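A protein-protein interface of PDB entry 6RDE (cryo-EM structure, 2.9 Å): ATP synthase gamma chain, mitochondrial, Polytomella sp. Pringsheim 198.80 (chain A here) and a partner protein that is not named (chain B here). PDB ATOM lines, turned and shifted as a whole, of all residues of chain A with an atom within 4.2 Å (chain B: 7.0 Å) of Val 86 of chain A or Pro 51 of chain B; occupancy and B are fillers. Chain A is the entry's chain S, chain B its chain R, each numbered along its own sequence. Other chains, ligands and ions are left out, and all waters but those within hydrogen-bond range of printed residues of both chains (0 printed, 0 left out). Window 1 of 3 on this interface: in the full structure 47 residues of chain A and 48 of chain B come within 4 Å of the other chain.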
ATOM      1  N   VAL A  82     -23.976  -8.661  -6.813  1.00  0.00           N
ATOM      2  CA  VAL A  82     -22.829  -9.189  -7.539  1.00  0.00           C
ATOM      3  C   VAL A  82     -22.259  -8.140  -8.481  1.00  0.00           C
ATOM      4  O   VAL A  82     -21.045  -8.082  -8.702  1.00  0.00           O
ATOM      5  CB  VAL A  82     -23.249 -10.466  -8.286  1.00  0.00           C
ATOM      6  CG1 VAL A  82     -22.058 -11.163  -8.920  1.00  0.00           C
ATOM      7  CG2 VAL A  82     -23.942 -11.392  -7.331  1.00  0.00           C
ATOM      8  N   ASP A  83     -23.119  -7.269  -9.011  1.00  0.00           N
ATOM      9  CA  ASP A  83     -22.699  -6.304 -10.029  1.00  0.00           C
ATOM     10  C   ASP A  83     -21.697  -5.240  -9.574  1.00  0.00           C
ATOM     11  O   ASP A  83     -20.775  -4.958 -10.357  1.00  0.00           O
ATOM     12  CB  ASP A  83     -23.932  -5.631 -10.647  1.00  0.00           C
ATOM     13  CG  ASP A  83     -25.047  -6.604 -10.927  1.00  0.00           C
ATOM     14  OD1 ASP A  83     -24.761  -7.693 -11.461  1.00  0.00           O
ATOM     15  OD2 ASP A  83     -26.213  -6.277 -10.627  1.00  0.00           O
ATOM     16  N   PRO A  84     -21.802  -4.594  -8.395  1.00  0.00           N
ATOM     17  CA  PRO A  84     -20.790  -3.582  -8.053  1.00  0.00           C
ATOM     18  C   PRO A  84     -19.404  -4.130  -7.807  1.00  0.00           C
ATOM     19  O   PRO A  84     -18.440  -3.366  -7.892  1.00  0.00           O
ATOM     20  CB  PRO A  84     -21.348  -2.940  -6.780  1.00  0.00           C
ATOM     21  CG  PRO A  84     -22.279  -3.874  -6.272  1.00  0.00           C
ATOM     22  CD  PRO A  84     -22.907  -4.499  -7.427  1.00  0.00           C
ATOM     23  N   PHE A  85     -19.262  -5.414  -7.514  1.00  0.00           N
ATOM     24  CA  PHE A  85     -17.933  -5.960  -7.307  1.00  0.00           C
ATOM     25  C   PHE A  85     -17.229  -6.279  -8.608  1.00  0.00           C
ATOM     26  O   PHE A  85     -16.003  -6.194  -8.674  1.00  0.00           O
ATOM     27  CB  PHE A  85     -18.013  -7.212  -6.456  1.00  0.00           C
ATOM     28  CG  PHE A  85     -18.307  -6.933  -5.039  1.00  0.00           C
ATOM     29  CD1 PHE A  85     -17.330  -6.416  -4.218  1.00  0.00           C
ATOM     30  CD2 PHE A  85     -19.562  -7.160  -4.529  1.00  0.00           C
ATOM     31  CE1 PHE A  85     -17.600  -6.145  -2.915  1.00  0.00           C
ATOM     32  CE2 PHE A  85     -19.836  -6.886  -3.232  1.00  0.00           C
ATOM     33  CZ  PHE A  85     -18.854  -6.382  -2.428  1.00  0.00           C
ATOM     34  N   VAL A  86     -17.969  -6.665  -9.643  1.00  0.00           N
ATOM     35  CA  VAL A  86     -17.337  -7.014 -10.905  1.00  0.00           C
ATOM     36  C   VAL A  86     -17.091  -5.801 -11.784  1.00  0.00           C
ATOM     37  O   VAL A  86     -16.470  -5.940 -12.849  1.00  0.00           O
ATOM     38  CB  VAL A  86     -18.170  -8.056 -11.672  1.00  0.00           C
ATOM     39  CG1 VAL A  86     -18.470  -9.234 -10.779  1.00  0.00           C
ATOM     40  CG2 VAL A  86     -19.440  -7.439 -12.159  1.00  0.00           C
ATOM     41  N   ARG A  87     -17.563  -4.622 -11.390  1.00  0.00           N
ATOM     42  CA  ARG A  87     -17.145  -3.399 -12.054  1.00  0.00           C
ATOM     43  C   ARG A  87     -16.122  -2.626 -11.241  1.00  0.00           C
ATOM     44  O   ARG A  87     -15.497  -1.708 -11.775  1.00  0.00           O
ATOM     45  CB  ARG A  87     -18.348  -2.502 -12.376  1.00  0.00           C
ATOM     46  CG  ARG A  87     -19.242  -2.122 -11.223  1.00  0.00           C
ATOM     47  CD  ARG A  87     -20.241  -1.077 -11.680  1.00  0.00           C
ATOM     48  NE  ARG A  87     -21.373  -0.935 -10.771  1.00  0.00           N
ATOM     49  CZ  ARG A  87     -22.590  -1.395 -11.023  1.00  0.00           C
ATOM     50  NH1 ARG A  87     -22.835  -2.027 -12.159  1.00  0.00           N
ATOM     51  NH2 ARG A  87     -23.563  -1.219 -10.146  1.00  0.00           N
ATOM     52  N   LEU A  88     -15.933  -2.982  -9.977  1.00  0.00           N
ATOM     53  CA  LEU A  88     -14.839  -2.452  -9.181  1.00  0.00           C
ATOM     54  C   LEU A  88     -13.577  -3.285  -9.312  1.00  0.00           C
ATOM     55  O   LEU A  88     -12.471  -2.741  -9.238  1.00  0.00           O
ATOM     56  CB  LEU A  88     -15.239  -2.396  -7.711  1.00  0.00           C
ATOM     57  CG  LEU A  88     -14.359  -1.499  -6.859  1.00  0.00           C
ATOM     58  CD1 LEU A  88     -14.756  -0.081  -7.121  1.00  0.00           C
ATOM     59  CD2 LEU A  88     -14.465  -1.842  -5.407  1.00  0.00           C
ATOM     60  N   GLY A  90     -13.346  -5.897 -11.868  1.00  0.00           N
ATOM     61  CA  GLY A  90     -13.260  -6.509 -13.175  1.00  0.00           C
ATOM     62  C   GLY A  90     -13.673  -7.968 -13.139  1.00  0.00           C
ATOM     63  O   GLY A  90     -14.457  -8.404 -12.291  1.00  0.00           O
ATOM     64  N   ASP A  91     -13.127  -8.737 -14.079  1.00  0.00           N
ATOM     65  CA  ASP A  91     -13.302 -10.186 -14.087  1.00  0.00           C
ATOM     66  C   ASP A  91     -12.097 -10.780 -14.805  1.00  0.00           C
ATOM     67  O   ASP A  91     -11.976 -10.642 -16.024  1.00  0.00           O
ATOM     68  CB  ASP A  91     -14.601 -10.586 -14.761  1.00  0.00           C
ATOM     69  CG  ASP A  91     -14.844 -12.072 -14.716  1.00  0.00           C
ATOM     70  OD1 ASP A  91     -15.293 -12.576 -13.667  1.00  0.00           O
ATOM     71  OD2 ASP A  91     -14.563 -12.739 -15.731  1.00  0.00           O
ATOM     72  N   THR A 206     -21.282 -20.958 -15.201  1.00  0.00           N
ATOM     73  CA  THR A 206     -20.528 -19.729 -15.056  1.00  0.00           C
ATOM     74  C   THR A 206     -19.249 -20.008 -14.288  1.00  0.00           C
ATOM     75  O   THR A 206     -19.246 -20.801 -13.343  1.00  0.00           O
ATOM     76  CB  THR A 206     -21.362 -18.681 -14.321  1.00  0.00           C
ATOM     77  OG1 THR A 206     -22.668 -18.630 -14.898  1.00  0.00           O
ATOM     78  CG2 THR A 206     -20.744 -17.307 -14.409  1.00  0.00           C
ATOM     79  N   VAL A 207     -18.158 -19.377 -14.712  1.00  0.00           N
ATOM     80  CA  VAL A 207     -16.941 -19.278 -13.919  1.00  0.00           C
ATOM     81  C   VAL A 207     -16.886 -17.880 -13.331  1.00  0.00           C
ATOM     82  O   VAL A 207     -16.781 -16.899 -14.073  1.00  0.00           O
ATOM     83  CB  VAL A 207     -15.681 -19.551 -14.754  1.00  0.00           C
ATOM     84  CG1 VAL A 207     -14.459 -19.366 -13.893  1.00  0.00           C
ATOM     85  CG2 VAL A 207     -15.702 -20.941 -15.318  1.00  0.00           C
ATOM     86  N   ALA A 208     -16.946 -17.788 -12.006  1.00  0.00           N
ATOM     87  CA  ALA A 208     -16.856 -16.516 -11.303  1.00  0.00           C
ATOM     88  C   ALA A 208     -15.623 -16.541 -10.421  1.00  0.00           C
ATOM     89  O   ALA A 208     -15.409 -17.502  -9.681  1.00  0.00           O
ATOM     90  CB  ALA A 208     -18.103 -16.257 -10.471  1.00  0.00           C
ATOM     91  N   GLU B  49     -19.526 -18.941 -19.283  1.00  0.00           N
ATOM     92  CA  GLU B  49     -19.785 -17.525 -19.119  1.00  0.00           C
ATOM     93  C   GLU B  49     -19.185 -17.011 -17.813  1.00  0.00           C
ATOM     94  O   GLU B  49     -18.686 -17.766 -16.979  1.00  0.00           O
ATOM     95  CB  GLU B  49     -21.277 -17.249 -19.200  1.00  0.00           C
ATOM     96  CG  GLU B  49     -21.843 -17.649 -20.538  1.00  0.00           C
ATOM     97  CD  GLU B  49     -23.050 -16.836 -20.933  1.00  0.00           C
ATOM     98  OE1 GLU B  49     -23.037 -15.611 -20.697  1.00  0.00           O
ATOM     99  OE2 GLU B  49     -24.018 -17.417 -21.466  1.00  0.00           O
ATOM    100  N   PHE B  50     -19.199 -15.694 -17.669  1.00  0.00           N
ATOM    101  CA  PHE B  50     -18.526 -14.977 -16.604  1.00  0.00           C
ATOM    102  C   PHE B  50     -19.465 -13.920 -16.051  1.00  0.00           C
ATOM    103  O   PHE B  50     -20.347 -13.448 -16.769  1.00  0.00           O
ATOM    104  CB  PHE B  50     -17.246 -14.312 -17.126  1.00  0.00           C
ATOM    105  CG  PHE B  50     -16.396 -15.214 -17.945  1.00  0.00           C
ATOM    106  CD1 PHE B  50     -16.406 -15.128 -19.321  1.00  0.00           C
ATOM    107  CD2 PHE B  50     -15.593 -16.161 -17.341  1.00  0.00           C
ATOM    108  CE1 PHE B  50     -15.624 -15.966 -20.082  1.00  0.00           C
ATOM    109  CE2 PHE B  50     -14.811 -17.002 -18.098  1.00  0.00           C
ATOM    110  CZ  PHE B  50     -14.826 -16.902 -19.468  1.00  0.00           C
ATOM    111  N   PRO B  51     -19.302 -13.522 -14.785  1.00  0.00           N
ATOM    112  CA  PRO B  51     -20.159 -12.460 -14.236  1.00  0.00           C
ATOM    113  C   PRO B  51     -19.945 -11.099 -14.871  1.00  0.00           C
ATOM    114  O   PRO B  51     -20.790 -10.217 -14.680  1.00  0.00           O
ATOM    115  CB  PRO B  51     -19.785 -12.440 -12.750  1.00  0.00           C
ATOM    116  CG  PRO B  51     -18.492 -13.140 -12.661  1.00  0.00           C
ATOM    117  CD  PRO B  51     -18.476 -14.142 -13.738  1.00  0.00           C
ATOM    118  N   SER B  52     -18.853 -10.902 -15.615  1.00  0.00           N
ATOM    119  CA  SER B  52     -18.670  -9.695 -16.408  1.00  0.00           C
ATOM    120  C   SER B  52     -19.689  -9.577 -17.528  1.00  0.00           C
ATOM    121  O   SER B  52     -20.060  -8.459 -17.895  1.00  0.00           O
ATOM    122  CB  SER B  52     -17.269  -9.674 -17.009  1.00  0.00           C
ATOM    123  OG  SER B  52     -17.087  -8.566 -17.869  1.00  0.00           O
ATOM    124  N   ASN B  53     -20.154 -10.704 -18.068  1.00  0.00           N
ATOM    125  CA  ASN B  53     -21.074 -10.709 -19.194  1.00  0.00           C
ATOM    126  C   ASN B  53     -22.483 -10.292 -18.810  1.00  0.00           C
ATOM    127  O   ASN B  53     -23.274  -9.962 -19.696  1.00  0.00           O
ATOM    128  CB  ASN B  53     -21.112 -12.099 -19.824  1.00  0.00           C
ATOM    129  CG  ASN B  53     -19.738 -12.701 -19.979  1.00  0.00           C
ATOM    130  OD1 ASN B  53     -19.494 -13.835 -19.578  1.00  0.00           O
ATOM    131  ND2 ASN B  53     -18.826 -11.942 -20.564  1.00  0.00           N
ATOM    132  N   TYR B  54     -22.818 -10.297 -17.524  1.00  0.00           N
ATOM    133  CA  TYR B  54     -24.178 -10.044 -17.085  1.00  0.00           C
ATOM    134  C   TYR B  54     -24.349  -8.670 -16.459  1.00  0.00           C
ATOM    135  O   TYR B  54     -25.373  -8.412 -15.819  1.00  0.00           O
ATOM    136  CB  TYR B  54     -24.618 -11.126 -16.104  1.00  0.00           C
ATOM    137  CG  TYR B  54     -24.521 -12.521 -16.662  1.00  0.00           C
ATOM    138  CD1 TYR B  54     -25.494 -13.013 -17.519  1.00  0.00           C
ATOM    139  CD2 TYR B  54     -23.466 -13.347 -16.321  1.00  0.00           C
ATOM    140  CE1 TYR B  54     -25.412 -14.288 -18.026  1.00  0.00           C
ATOM    141  CE2 TYR B  54     -23.366 -14.616 -16.827  1.00  0.00           C
ATOM    142  CZ  TYR B  54     -24.344 -15.085 -17.672  1.00  0.00           C
ATOM    143  OH  TYR B  54     -24.257 -16.361 -18.162  1.00  0.00           O
ATOM    144  N   THR B  55     -23.371  -7.784 -16.624  1.00  0.00           N
ATOM    145  CA  THR B  55     -23.479  -6.400 -16.184  1.00  0.00           C
ATOM    146  C   THR B  55     -23.362  -5.475 -17.382  1.00  0.00           C
ATOM    147  O   THR B  55     -22.437  -5.610 -18.190  1.00  0.00           O
ATOM    148  CB  THR B  55     -22.411  -6.059 -15.152  1.00  0.00           C
ATOM    149  OG1 THR B  55     -21.120  -6.364 -15.692  1.00  0.00           O
ATOM    150  CG2 THR B  55     -22.632  -6.851 -13.899  1.00  0.00           C
ATOM    151  N   VAL B  57     -23.370  -2.004 -16.963  1.00  0.00           N
ATOM    152  CA  VAL B  57     -22.774  -0.751 -16.516  1.00  0.00           C
ATOM    153  C   VAL B  57     -21.403  -1.063 -15.935  1.00  0.00           C
ATOM    154  O   VAL B  57     -21.298  -1.783 -14.935  1.00  0.00           O
ATOM    155  CB  VAL B  57     -23.653  -0.039 -15.477  1.00  0.00           C
ATOM    156  CG1 VAL B  57     -23.000   1.261 -15.038  1.00  0.00           C
ATOM    157  CG2 VAL B  57     -25.045   0.208 -16.021  1.00  0.00           C
ATOM    158  N   LYS B  58     -20.356  -0.527 -16.558  1.00  0.00           N
ATOM    159  CA  LYS B  58     -19.003  -0.602 -16.032  1.00  0.00           C
ATOM    160  C   LYS B  58     -18.654   0.695 -15.302  1.00  0.00           C
ATOM    161  O   LYS B  58     -19.519   1.517 -14.991  1.00  0.00           O
ATOM    162  CB  LYS B  58     -18.001  -0.916 -17.141  1.00  0.00           C
ATOM    163  CG  LYS B  58     -18.192  -2.280 -17.761  1.00  0.00           C
ATOM    164  CD  LYS B  58     -17.975  -3.371 -16.727  1.00  0.00           C
ATOM    165  CE  LYS B  58     -18.061  -4.752 -17.349  1.00  0.00           C
ATOM    166  NZ  LYS B  58     -19.447  -5.094 -17.773  1.00  0.00           N
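Asp 83 of chain A touches Thr 55 of chain B.
Pro 51 of chain B touches Val 86 of chain A.
Phe 50 of chain B touches Asp 91 of chain A (CB to OD2, 3.4 Å).
Pro 51 of chain B touches Asp 91 of chain A (CG to OD1, 3.4 Å).
O of Glu 49 of chain B touches CA of Thr 206 of chain A, 3.3 Å away.
CG2 of Thr 206 of chain A touches CA of Phe 50 of chain B (3.9 Å).
Thr 206 of chain A touches Pro 51 of chain B (CG2 to CD, 3.95 Å).
Val 207 of chain A touches Phe 50 of chain B (O to CD2, 3.6 Å).
O of Val 207 of chain A touches CD of Pro 51 of chain B, 3.3 Å away.
Ala 208 of chain A touches Pro 51 of chain B.
Printed residues of chain A that touch a printed residue of chain B: Asp 83, Val 86, Arg 87, Asp 91, Thr 206, Val 207 and Ala 208.
Of the 9 printed residues of chain B, 6 touch a printed residue of chain A.
Printed residues of chain B that touch a printed residue of chain A: Glu 49, Phe 50, Pro 51, Ser 52, Thr 55 and Val 57.
Among the printed residues, no Asp or Glu carboxylate lies within 4 Å of a Lys or Arg side-chain nitrogen of the other chain.
The backbone NH (N) of Val 207 of chain A lies within hydrogen-bond range of the backbone carbonyl oxygen (O) of Glu 49 of chain B (2.8 Å).
The backbone carbonyl oxygen (O) of Val 57 of chain B lies within hydrogen-bond range of the guanidinium group (NH1) of Arg 87 of chain A (3.2 Å).
Of the printed residues of chain B, Val 86 of chain A touches Pro 51 and Thr 55.
Of the printed residues of chain B, Ala 208 of chain A touches Pro 51 (3.8 Å).
Printed residues of chain B within 4 Å of Thr 206 of chain A: Glu 49, Phe 50 and Pro 51.
Val 82 of chain A touches none of the printed residues of chain B.
Asn 53 of chain B touches none of the printed residues of chain A.
The nearest printed residue of chain A that does not touch Pro 51 of chain B is Val 82 of chain A (4.6 Å).
The backbone carbonyl oxygen (O) of Ser 52 of chain B sits at hydrogen-bond distance from the side-chain amino group (NZ) of Lys 58 of chain B (3.4 Å).
The side-chain hydroxyl of Thr 55 of chain B lies within hydrogen-bond range of the side-chain amino group of Lys 58 of chain B (3.0 Å).
The backbone NH (N) of Phe 50 of chain B lies within hydrogen-bond range of the side-chain amide oxygen (OD1) of Asn 53 of chain B.
The side-chain carboxylate of Glu 49 of chain B is in hydrogen-bond range of the side-chain hydroxyl of Tyr 54 of chain B.
The side-chain hydroxyl (OG1) of Thr 55 of chain B lies within hydrogen-bond range of the backbone carbonyl oxygen (O) of Ser 52 of chain B, 3.2 Å away.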
